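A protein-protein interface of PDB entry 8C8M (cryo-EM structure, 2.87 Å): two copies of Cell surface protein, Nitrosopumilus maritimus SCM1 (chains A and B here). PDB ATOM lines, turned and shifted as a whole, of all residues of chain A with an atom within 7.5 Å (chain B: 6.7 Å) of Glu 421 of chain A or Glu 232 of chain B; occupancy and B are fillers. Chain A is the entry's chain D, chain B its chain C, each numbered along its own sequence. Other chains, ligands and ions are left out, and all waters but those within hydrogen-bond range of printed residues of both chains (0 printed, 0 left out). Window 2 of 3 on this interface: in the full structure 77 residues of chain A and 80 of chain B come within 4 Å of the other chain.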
ATOM      1  N   GLU A 321       7.227 -27.942  -1.498  1.00  0.00           N
ATOM      2  CA  GLU A 321       7.651 -27.470  -2.843  1.00  0.00           C
ATOM      3  C   GLU A 321       7.505 -25.946  -2.949  1.00  0.00           C
ATOM      4  O   GLU A 321       7.935 -25.402  -3.960  1.00  0.00           O
ATOM      5  CB  GLU A 321       6.885 -28.177  -3.962  1.00  0.00           C
ATOM      6  CG  GLU A 321       5.407 -27.829  -4.088  1.00  0.00           C
ATOM      7  CD  GLU A 321       4.486 -28.730  -3.300  1.00  0.00           C
ATOM      8  OE1 GLU A 321       5.005 -29.524  -2.503  1.00  0.00           O
ATOM      9  OE2 GLU A 321       3.251 -28.645  -3.450  1.00  0.00           O
ATOM     10  N   ASN A 322       6.930 -25.301  -1.941  1.00  0.00           N
ATOM     11  CA  ASN A 322       6.721 -23.837  -1.870  1.00  0.00           C
ATOM     12  C   ASN A 322       7.638 -23.211  -0.803  1.00  0.00           C
ATOM     13  O   ASN A 322       7.394 -22.040  -0.428  1.00  0.00           O
ATOM     14  CB  ASN A 322       5.263 -23.555  -1.550  1.00  0.00           C
ATOM     15  CG  ASN A 322       4.330 -24.357  -2.429  1.00  0.00           C
ATOM     16  OD1 ASN A 322       4.681 -24.666  -3.565  1.00  0.00           O
ATOM     17  ND2 ASN A 322       3.185 -24.749  -1.894  1.00  0.00           N
ATOM     18  N   ASN A 366      16.890 -20.372  -1.309  1.00  0.00           N
ATOM     19  CA  ASN A 366      16.112 -20.182  -2.555  1.00  0.00           C
ATOM     20  C   ASN A 366      14.631 -20.309  -2.210  1.00  0.00           C
ATOM     21  O   ASN A 366      14.299 -20.261  -1.003  1.00  0.00           O
ATOM     22  CB  ASN A 366      16.588 -21.122  -3.664  1.00  0.00           C
ATOM     23  CG  ASN A 366      16.282 -22.576  -3.368  1.00  0.00           C
ATOM     24  OD1 ASN A 366      15.754 -22.915  -2.300  1.00  0.00           O
ATOM     25  ND2 ASN A 366      16.619 -23.448  -4.305  1.00  0.00           N
ATOM     26  N   GLY A 367      13.787 -20.438  -3.245  1.00  0.00           N
ATOM     27  CA  GLY A 367      12.317 -20.432  -3.136  1.00  0.00           C
ATOM     28  C   GLY A 367      11.728 -21.748  -2.655  1.00  0.00           C
ATOM     29  O   GLY A 367      10.517 -21.788  -2.418  1.00  0.00           O
ATOM     30  N   ASP A 368      12.523 -22.807  -2.552  1.00  0.00           N
ATOM     31  CA  ASP A 368      12.015 -24.153  -2.200  1.00  0.00           C
ATOM     32  C   ASP A 368      12.678 -24.627  -0.914  1.00  0.00           C
ATOM     33  O   ASP A 368      12.689 -25.841  -0.688  1.00  0.00           O
ATOM     34  CB  ASP A 368      12.315 -25.128  -3.336  1.00  0.00           C
ATOM     35  CG  ASP A 368      11.502 -24.855  -4.588  1.00  0.00           C
ATOM     36  OD1 ASP A 368      10.291 -24.559  -4.440  1.00  0.00           O
ATOM     37  OD2 ASP A 368      12.076 -24.945  -5.696  1.00  0.00           O
ATOM     38  N   THR A 407      13.997 -30.680  -5.096  1.00  0.00           N
ATOM     39  CA  THR A 407      12.528 -30.621  -5.264  1.00  0.00           C
ATOM     40  C   THR A 407      12.156 -31.292  -6.572  1.00  0.00           C
ATOM     41  O   THR A 407      12.946 -31.221  -7.551  1.00  0.00           O
ATOM     42  CB  THR A 407      12.023 -29.180  -5.214  1.00  0.00           C
ATOM     43  OG1 THR A 407      12.328 -28.628  -3.931  1.00  0.00           O
ATOM     44  CG2 THR A 407      10.531 -29.082  -5.444  1.00  0.00           C
ATOM     45  N   GLU A 408      11.000 -31.930  -6.583  1.00  0.00           N
ATOM     46  CA  GLU A 408      10.529 -32.731  -7.746  1.00  0.00           C
ATOM     47  C   GLU A 408       9.979 -31.763  -8.808  1.00  0.00           C
ATOM     48  O   GLU A 408       9.081 -30.944  -8.506  1.00  0.00           O
ATOM     49  CB  GLU A 408       9.506 -33.758  -7.252  1.00  0.00           C
ATOM     50  CG  GLU A 408       9.301 -34.975  -8.138  1.00  0.00           C
ATOM     51  CD  GLU A 408       7.988 -35.669  -7.793  1.00  0.00           C
ATOM     52  OE1 GLU A 408       7.158 -34.948  -7.213  1.00  0.00           O
ATOM     53  OE2 GLU A 408       7.728 -36.853  -8.148  1.00  0.00           O
ATOM     54  N   GLN A 409      10.481 -31.878 -10.032  1.00  0.00           N
ATOM     55  CA  GLN A 409      10.030 -31.095 -11.213  1.00  0.00           C
ATOM     56  C   GLN A 409       8.738 -31.717 -11.775  1.00  0.00           C
ATOM     57  O   GLN A 409       8.790 -32.337 -12.855  1.00  0.00           O
ATOM     58  CB  GLN A 409      11.163 -31.067 -12.251  1.00  0.00           C
ATOM     59  CG  GLN A 409      12.440 -30.360 -11.795  1.00  0.00           C
ATOM     60  CD  GLN A 409      12.173 -29.098 -11.009  1.00  0.00           C
ATOM     61  OE1 GLN A 409      11.348 -28.275 -11.404  1.00  0.00           O
ATOM     62  NE2 GLN A 409      12.870 -28.925  -9.891  1.00  0.00           N
ATOM     63  N   THR A 418      18.126 -28.808  -7.886  1.00  0.00           N
ATOM     64  CA  THR A 418      18.461 -27.781  -6.874  1.00  0.00           C
ATOM     65  C   THR A 418      17.982 -26.397  -7.305  1.00  0.00           C
ATOM     66  O   THR A 418      17.831 -25.581  -6.433  1.00  0.00           O
ATOM     67  CB  THR A 418      19.955 -27.805  -6.602  1.00  0.00           C
ATOM     68  OG1 THR A 418      20.640 -27.779  -7.858  1.00  0.00           O
ATOM     69  CG2 THR A 418      20.345 -29.044  -5.835  1.00  0.00           C
ATOM     70  N   TYR A 419      17.651 -26.176  -8.576  1.00  0.00           N
ATOM     71  CA  TYR A 419      17.105 -24.872  -9.046  1.00  0.00           C
ATOM     72  C   TYR A 419      15.676 -24.683  -8.538  1.00  0.00           C
ATOM     73  O   TYR A 419      14.999 -25.651  -8.236  1.00  0.00           O
ATOM     74  CB  TYR A 419      17.176 -24.711 -10.562  1.00  0.00           C
ATOM     75  CG  TYR A 419      17.046 -25.975 -11.359  1.00  0.00           C
ATOM     76  CD1 TYR A 419      18.158 -26.741 -11.651  1.00  0.00           C
ATOM     77  CD2 TYR A 419      15.819 -26.398 -11.835  1.00  0.00           C
ATOM     78  CE1 TYR A 419      18.050 -27.899 -12.403  1.00  0.00           C
ATOM     79  CE2 TYR A 419      15.699 -27.534 -12.615  1.00  0.00           C
ATOM     80  CZ  TYR A 419      16.816 -28.303 -12.886  1.00  0.00           C
ATOM     81  OH  TYR A 419      16.709 -29.441 -13.636  1.00  0.00           O
ATOM     82  N   ASP A 420      15.242 -23.435  -8.444  1.00  0.00           N
ATOM     83  CA  ASP A 420      13.838 -23.056  -8.141  1.00  0.00           C
ATOM     84  C   ASP A 420      13.245 -22.396  -9.390  1.00  0.00           C
ATOM     85  O   ASP A 420      13.819 -22.526 -10.482  1.00  0.00           O
ATOM     86  CB  ASP A 420      13.789 -22.211  -6.872  1.00  0.00           C
ATOM     87  CG  ASP A 420      14.310 -20.791  -7.045  1.00  0.00           C
ATOM     88  OD1 ASP A 420      14.944 -20.503  -8.100  1.00  0.00           O
ATOM     89  OD2 ASP A 420      14.091 -19.981  -6.117  1.00  0.00           O
ATOM     90  N   GLU A 421      12.066 -21.787  -9.299  1.00  0.00           N
ATOM     91  CA  GLU A 421      11.381 -21.292 -10.522  1.00  0.00           C
ATOM     92  C   GLU A 421      12.015 -19.987 -10.978  1.00  0.00           C
ATOM     93  O   GLU A 421      11.885 -19.703 -12.147  1.00  0.00           O
ATOM     94  CB  GLU A 421       9.879 -21.146 -10.311  1.00  0.00           C
ATOM     95  CG  GLU A 421       9.109 -22.463 -10.403  1.00  0.00           C
ATOM     96  CD  GLU A 421       9.461 -23.584  -9.434  1.00  0.00           C
ATOM     97  OE1 GLU A 421       9.100 -23.480  -8.257  1.00  0.00           O
ATOM     98  OE2 GLU A 421      10.120 -24.557  -9.868  1.00  0.00           O
ATOM     99  N   SER A 422      12.736 -19.277 -10.116  1.00  0.00           N
ATOM    100  CA  SER A 422      13.487 -18.054 -10.505  1.00  0.00           C
ATOM    101  C   SER A 422      14.891 -18.405 -11.024  1.00  0.00           C
ATOM    102  O   SER A 422      15.675 -17.475 -11.266  1.00  0.00           O
ATOM    103  CB  SER A 422      13.554 -17.111  -9.363  1.00  0.00           C
ATOM    104  OG  SER A 422      12.411 -17.262  -8.535  1.00  0.00           O
ATOM    105  N   ASP A 423      15.214 -19.691 -11.136  1.00  0.00           N
ATOM    106  CA  ASP A 423      16.527 -20.227 -11.580  1.00  0.00           C
ATOM    107  C   ASP A 423      17.621 -19.946 -10.533  1.00  0.00           C
ATOM    108  O   ASP A 423      18.803 -19.875 -10.940  1.00  0.00           O
ATOM    109  CB  ASP A 423      16.838 -19.738 -12.994  1.00  0.00           C
ATOM    110  CG  ASP A 423      15.951 -20.380 -14.038  1.00  0.00           C
ATOM    111  OD1 ASP A 423      15.744 -21.612 -13.947  1.00  0.00           O
ATOM    112  OD2 ASP A 423      15.493 -19.656 -14.958  1.00  0.00           O
ATOM    113  N   LYS A 424      17.286 -19.870  -9.240  1.00  0.00           N
ATOM    114  CA  LYS A 424      18.304 -19.681  -8.177  1.00  0.00           C
ATOM    115  C   LYS A 424      18.615 -21.039  -7.535  1.00  0.00           C
ATOM    116  O   LYS A 424      17.855 -21.509  -6.683  1.00  0.00           O
ATOM    117  CB  LYS A 424      17.868 -18.649  -7.130  1.00  0.00           C
ATOM    118  CG  LYS A 424      18.921 -18.372  -6.063  1.00  0.00           C
ATOM    119  CD  LYS A 424      18.895 -16.999  -5.491  1.00  0.00           C
ATOM    120  CE  LYS A 424      17.972 -16.868  -4.309  1.00  0.00           C
ATOM    121  NZ  LYS A 424      18.674 -16.351  -3.103  1.00  0.00           N
ATOM    122  N   ARG A 488      20.495 -21.190 -17.220  1.00  0.00           N
ATOM    123  CA  ARG A 488      19.026 -21.235 -17.398  1.00  0.00           C
ATOM    124  C   ARG A 488      18.444 -19.830 -17.504  1.00  0.00           C
ATOM    125  O   ARG A 488      17.233 -19.692 -17.400  1.00  0.00           O
ATOM    126  CB  ARG A 488      18.401 -21.984 -16.227  1.00  0.00           C
ATOM    127  CG  ARG A 488      18.929 -23.399 -16.085  1.00  0.00           C
ATOM    128  CD  ARG A 488      18.444 -23.966 -14.755  1.00  0.00           C
ATOM    129  NE  ARG A 488      16.992 -23.985 -14.665  1.00  0.00           N
ATOM    130  CZ  ARG A 488      16.202 -24.759 -15.414  1.00  0.00           C
ATOM    131  NH1 ARG A 488      16.704 -25.596 -16.309  1.00  0.00           N
ATOM    132  NH2 ARG A 488      14.898 -24.760 -15.194  1.00  0.00           N
ATOM    133  N   ASN B  84       1.428 -27.588 -15.891  1.00  0.00           N
ATOM    134  CA  ASN B  84       2.724 -28.082 -15.353  1.00  0.00           C
ATOM    135  C   ASN B  84       2.495 -29.171 -14.293  1.00  0.00           C
ATOM    136  O   ASN B  84       3.225 -29.207 -13.279  1.00  0.00           O
ATOM    137  CB  ASN B  84       3.552 -26.945 -14.755  1.00  0.00           C
ATOM    138  CG  ASN B  84       4.000 -25.958 -15.811  1.00  0.00           C
ATOM    139  OD1 ASN B  84       3.586 -24.798 -15.776  1.00  0.00           O
ATOM    140  ND2 ASN B  84       4.784 -26.409 -16.782  1.00  0.00           N
ATOM    141  N   LYS B  86       0.044 -29.545 -12.233  1.00  0.00           N
ATOM    142  CA  LYS B  86      -0.809 -29.150 -11.074  1.00  0.00           C
ATOM    143  C   LYS B  86      -2.257 -28.921 -11.507  1.00  0.00           C
ATOM    144  O   LYS B  86      -2.459 -28.382 -12.595  1.00  0.00           O
ATOM    145  CB  LYS B  86      -0.243 -27.885 -10.456  1.00  0.00           C
ATOM    146  CG  LYS B  86       1.114 -28.091  -9.835  1.00  0.00           C
ATOM    147  CD  LYS B  86       1.668 -26.821  -9.257  1.00  0.00           C
ATOM    148  CE  LYS B  86       2.003 -25.771 -10.295  1.00  0.00           C
ATOM    149  NZ  LYS B  86       3.186 -26.169 -11.077  1.00  0.00           N
ATOM    150  N   ALA B 103      -2.813 -17.408 -14.128  1.00  0.00           N
ATOM    151  CA  ALA B 103      -1.745 -16.414 -14.375  1.00  0.00           C
ATOM    152  C   ALA B 103      -0.523 -16.699 -13.506  1.00  0.00           C
ATOM    153  O   ALA B 103      -0.632 -17.401 -12.502  1.00  0.00           O
ATOM    154  CB  ALA B 103      -2.270 -15.053 -14.100  1.00  0.00           C
ATOM    155  N   ASP B 104       0.620 -16.171 -13.908  1.00  0.00           N
ATOM    156  CA  ASP B 104       1.870 -16.225 -13.108  1.00  0.00           C
ATOM    157  C   ASP B 104       1.655 -15.469 -11.797  1.00  0.00           C
ATOM    158  O   ASP B 104       1.039 -14.389 -11.817  1.00  0.00           O
ATOM    159  CB  ASP B 104       3.066 -15.692 -13.885  1.00  0.00           C
ATOM    160  CG  ASP B 104       4.348 -15.626 -13.067  1.00  0.00           C
ATOM    161  OD1 ASP B 104       5.422 -15.770 -13.674  1.00  0.00           O
ATOM    162  OD2 ASP B 104       4.285 -15.378 -11.836  1.00  0.00           O
ATOM    163  N   ARG B 105       2.177 -16.015 -10.701  1.00  0.00           N
ATOM    164  CA  ARG B 105       1.966 -15.454  -9.347  1.00  0.00           C
ATOM    165  C   ARG B 105       2.616 -14.065  -9.251  1.00  0.00           C
ATOM    166  O   ARG B 105       1.945 -13.134  -8.778  1.00  0.00           O
ATOM    167  CB  ARG B 105       2.487 -16.410  -8.275  1.00  0.00           C
ATOM    168  CG  ARG B 105       2.253 -15.873  -6.870  1.00  0.00           C
ATOM    169  CD  ARG B 105       2.980 -16.686  -5.839  1.00  0.00           C
ATOM    170  NE  ARG B 105       4.409 -16.702  -6.062  1.00  0.00           N
ATOM    171  CZ  ARG B 105       5.271 -17.481  -5.418  1.00  0.00           C
ATOM    172  NH1 ARG B 105       4.852 -18.337  -4.495  1.00  0.00           N
ATOM    173  NH2 ARG B 105       6.560 -17.420  -5.728  1.00  0.00           N
ATOM    174  N   ASP B 106       3.882 -13.939  -9.635  1.00  0.00           N
ATOM    175  CA  ASP B 106       4.650 -12.699  -9.380  1.00  0.00           C
ATOM    176  C   ASP B 106       4.135 -11.594 -10.298  1.00  0.00           C
ATOM    177  O   ASP B 106       3.967 -10.472  -9.835  1.00  0.00           O
ATOM    178  CB  ASP B 106       6.136 -12.953  -9.548  1.00  0.00           C
ATOM    179  CG  ASP B 106       6.719 -13.817  -8.437  1.00  0.00           C
ATOM    180  OD1 ASP B 106       7.557 -14.699  -8.748  1.00  0.00           O
ATOM    181  OD2 ASP B 106       6.359 -13.591  -7.267  1.00  0.00           O
ATOM    182  N   GLN B 109       0.833 -10.174  -8.890  1.00  0.00           N
ATOM    183  CA  GLN B 109       1.129  -9.356  -7.683  1.00  0.00           C
ATOM    184  C   GLN B 109       1.717  -8.015  -8.119  1.00  0.00           C
ATOM    185  O   GLN B 109       1.294  -6.998  -7.604  1.00  0.00           O
ATOM    186  CB  GLN B 109       2.088 -10.078  -6.745  1.00  0.00           C
ATOM    187  CG  GLN B 109       1.417 -11.197  -5.987  1.00  0.00           C
ATOM    188  CD  GLN B 109       2.353 -11.814  -4.990  1.00  0.00           C
ATOM    189  OE1 GLN B 109       2.298 -11.526  -3.801  1.00  0.00           O
ATOM    190  NE2 GLN B 109       3.238 -12.655  -5.476  1.00  0.00           N
ATOM    191  N   ASP B 145      -0.614 -21.957  -6.321  1.00  0.00           N
ATOM    192  CA  ASP B 145       0.278 -21.051  -5.563  1.00  0.00           C
ATOM    193  C   ASP B 145      -0.527 -19.964  -4.866  1.00  0.00           C
ATOM    194  O   ASP B 145      -0.039 -19.465  -3.859  1.00  0.00           O
ATOM    195  CB  ASP B 145       1.366 -20.504  -6.472  1.00  0.00           C
ATOM    196  CG  ASP B 145       2.296 -21.632  -6.918  1.00  0.00           C
ATOM    197  OD1 ASP B 145       2.560 -22.550  -6.106  1.00  0.00           O
ATOM    198  OD2 ASP B 145       2.769 -21.599  -8.073  1.00  0.00           O
ATOM    199  N   GLY B 171       6.366 -12.507  -4.584  1.00  0.00           N
ATOM    200  CA  GLY B 171       6.787 -13.512  -3.602  1.00  0.00           C
ATOM    201  C   GLY B 171       5.654 -14.433  -3.243  1.00  0.00           C
ATOM    202  O   GLY B 171       4.679 -14.524  -4.013  1.00  0.00           O
ATOM    203  N   LEU B 230      -3.333 -18.831  -9.218  1.00  0.00           N
ATOM    204  CA  LEU B 230      -1.958 -18.333  -9.435  1.00  0.00           C
ATOM    205  C   LEU B 230      -0.989 -19.515  -9.483  1.00  0.00           C
ATOM    206  O   LEU B 230      -1.092 -20.402  -8.638  1.00  0.00           O
ATOM    207  CB  LEU B 230      -1.597 -17.315  -8.354  1.00  0.00           C
ATOM    208  CG  LEU B 230      -2.075 -15.889  -8.635  1.00  0.00           C
ATOM    209  CD1 LEU B 230      -1.563 -15.402  -9.995  1.00  0.00           C
ATOM    210  CD2 LEU B 230      -3.576 -15.788  -8.621  1.00  0.00           C
ATOM    211  N   TYR B 231      -0.066 -19.517 -10.446  1.00  0.00           N
ATOM    212  CA  TYR B 231       0.983 -20.554 -10.535  1.00  0.00           C
ATOM    213  C   TYR B 231       2.361 -19.920 -10.682  1.00  0.00           C
ATOM    214  O   TYR B 231       2.514 -18.968 -11.441  1.00  0.00           O
ATOM    215  CB  TYR B 231       0.706 -21.474 -11.711  1.00  0.00           C
ATOM    216  CG  TYR B 231      -0.527 -22.315 -11.541  1.00  0.00           C
ATOM    217  CD1 TYR B 231      -1.604 -22.216 -12.428  1.00  0.00           C
ATOM    218  CD2 TYR B 231      -0.614 -23.205 -10.483  1.00  0.00           C
ATOM    219  CE1 TYR B 231      -2.742 -22.977 -12.240  1.00  0.00           C
ATOM    220  CE2 TYR B 231      -1.744 -23.984 -10.295  1.00  0.00           C
ATOM    221  CZ  TYR B 231      -2.799 -23.880 -11.194  1.00  0.00           C
ATOM    222  OH  TYR B 231      -3.926 -24.618 -11.047  1.00  0.00           O
ATOM    223  N   GLU B 232       3.357 -20.491 -10.019  1.00  0.00           N
ATOM    224  CA  GLU B 232       4.758 -20.034 -10.115  1.00  0.00           C
ATOM    225  C   GLU B 232       5.373 -20.656 -11.374  1.00  0.00           C
ATOM    226  O   GLU B 232       5.549 -21.862 -11.425  1.00  0.00           O
ATOM    227  CB  GLU B 232       5.536 -20.360  -8.843  1.00  0.00           C
ATOM    228  CG  GLU B 232       6.929 -19.774  -8.830  1.00  0.00           C
ATOM    229  CD  GLU B 232       7.033 -18.257  -8.948  1.00  0.00           C
ATOM    230  OE1 GLU B 232       6.131 -17.563  -8.456  1.00  0.00           O
ATOM    231  OE2 GLU B 232       8.044 -17.764  -9.529  1.00  0.00           O
ATOM    232  N   LEU B 233       5.675 -19.842 -12.366  1.00  0.00           N
ATOM    233  CA  LEU B 233       6.108 -20.320 -13.692  1.00  0.00           C
ATOM    234  C   LEU B 233       7.554 -19.892 -13.953  1.00  0.00           C
ATOM    235  O   LEU B 233       8.043 -18.935 -13.295  1.00  0.00           O
ATOM    236  CB  LEU B 233       5.167 -19.729 -14.749  1.00  0.00           C
ATOM    237  CG  LEU B 233       3.680 -20.089 -14.670  1.00  0.00           C
ATOM    238  CD1 LEU B 233       2.912 -19.239 -15.682  1.00  0.00           C
ATOM    239  CD2 LEU B 233       3.420 -21.573 -14.945  1.00  0.00           C
ATOM    240  N   ASN B 234       8.212 -20.550 -14.895  1.00  0.00           N
ATOM    241  CA  ASN B 234       9.660 -20.346 -15.116  1.00  0.00           C
ATOM    242  C   ASN B 234       9.830 -19.497 -16.353  1.00  0.00           C
ATOM    243  O   ASN B 234       9.468 -19.926 -17.439  1.00  0.00           O
ATOM    244  CB  ASN B 234      10.410 -21.669 -15.250  1.00  0.00           C
ATOM    245  CG  ASN B 234      11.908 -21.502 -15.388  1.00  0.00           C
ATOM    246  OD1 ASN B 234      12.516 -21.990 -16.334  1.00  0.00           O
ATOM    247  ND2 ASN B 234      12.533 -20.844 -14.430  1.00  0.00           N
ATOM    248  N   PRO B 235      10.324 -18.251 -16.232  1.00  0.00           N
ATOM    249  CA  PRO B 235      10.664 -17.453 -17.411  1.00  0.00           C
ATOM    250  C   PRO B 235      11.642 -18.164 -18.355  1.00  0.00           C
ATOM    251  O   PRO B 235      12.568 -18.821 -17.906  1.00  0.00           O
ATOM    252  CB  PRO B 235      11.340 -16.209 -16.850  1.00  0.00           C
ATOM    253  CG  PRO B 235      10.873 -16.132 -15.420  1.00  0.00           C
ATOM    254  CD  PRO B 235      10.463 -17.516 -14.973  1.00  0.00           C
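Asn 322 of chain A touches Asp 145 of chain B (OD1 to OD1, 3.9 Å). Glu 421 of chain A touches Glu 232 of chain B. Glu 421 of chain A touches Pro 235 of chain B (O to CD, 3.8 Å). Arg 488 of chain A touches Asn 234 of chain B.
No position is printed for both chains.
O of Leu 230 of chain B lies within hydrogen-bond range of N of Asp 145 of chain B (2.8 Å). The side-chain carboxylate (OD1) of Asp 423 of chain A is in salt-bridge range of the guanidinium group (NE) of Arg 488 of chain A (2.8 Å). OE1 of Glu 232 of chain B lies within salt-bridge range of NH2 of Arg 105 of chain B. The side-chain carboxylate (OD1) of Asp 420 of chain A is in hydrogen-bond range of the backbone NH (N) of Asp 423 of chain A (3.2 Å).
The side-chain amide nitrogen (ND2) of Asn 234 of chain B lies within hydrogen-bond range of the side-chain carboxylate (OD2) of Asp 423 of chain A. The backbone carbonyl oxygen of Glu 421 of chain A is in hydrogen-bond range of the side-chain amide nitrogen of Asn 234 of chain B.
Of the printed residues of chain B, Asn 322 of chain A touches Asp 145 (3.9 Å). Glu 421 of chain A touches just these residues of chain B: Glu 232, Asn 234 and Pro 235. Printed residues of chain B within 4 Å of Asp 423 of chain A: Asn 234 (3.2 Å). Of the printed residues of chain A, Asp 145 of chain B touches Asn 322 (3.9 Å). Of chain A, only Glu 421 (3.6 Å) comes within 4 Å of Glu 232 of chain B. Of the printed residues of chain A, Asn 234 of chain B touches Glu 421 (2.6 Å), Asp 423 (3.2 Å) and Arg 488 (3.8 Å). The nearest residue of chain A that does not touch Glu 232 of chain B is Ser 422 of chain A (4.5 Å).
Of the 15 printed residues of chain B, 4 touch a printed residue of chain A. Hydrophobic or aromatic side chains of chain B within 4 Å of the printed part of chain A: Pro 235. Among the printed residues, no Asp or Glu carboxylate lies within 4 Å of a Lys or Arg side-chain nitrogen of the other chain.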
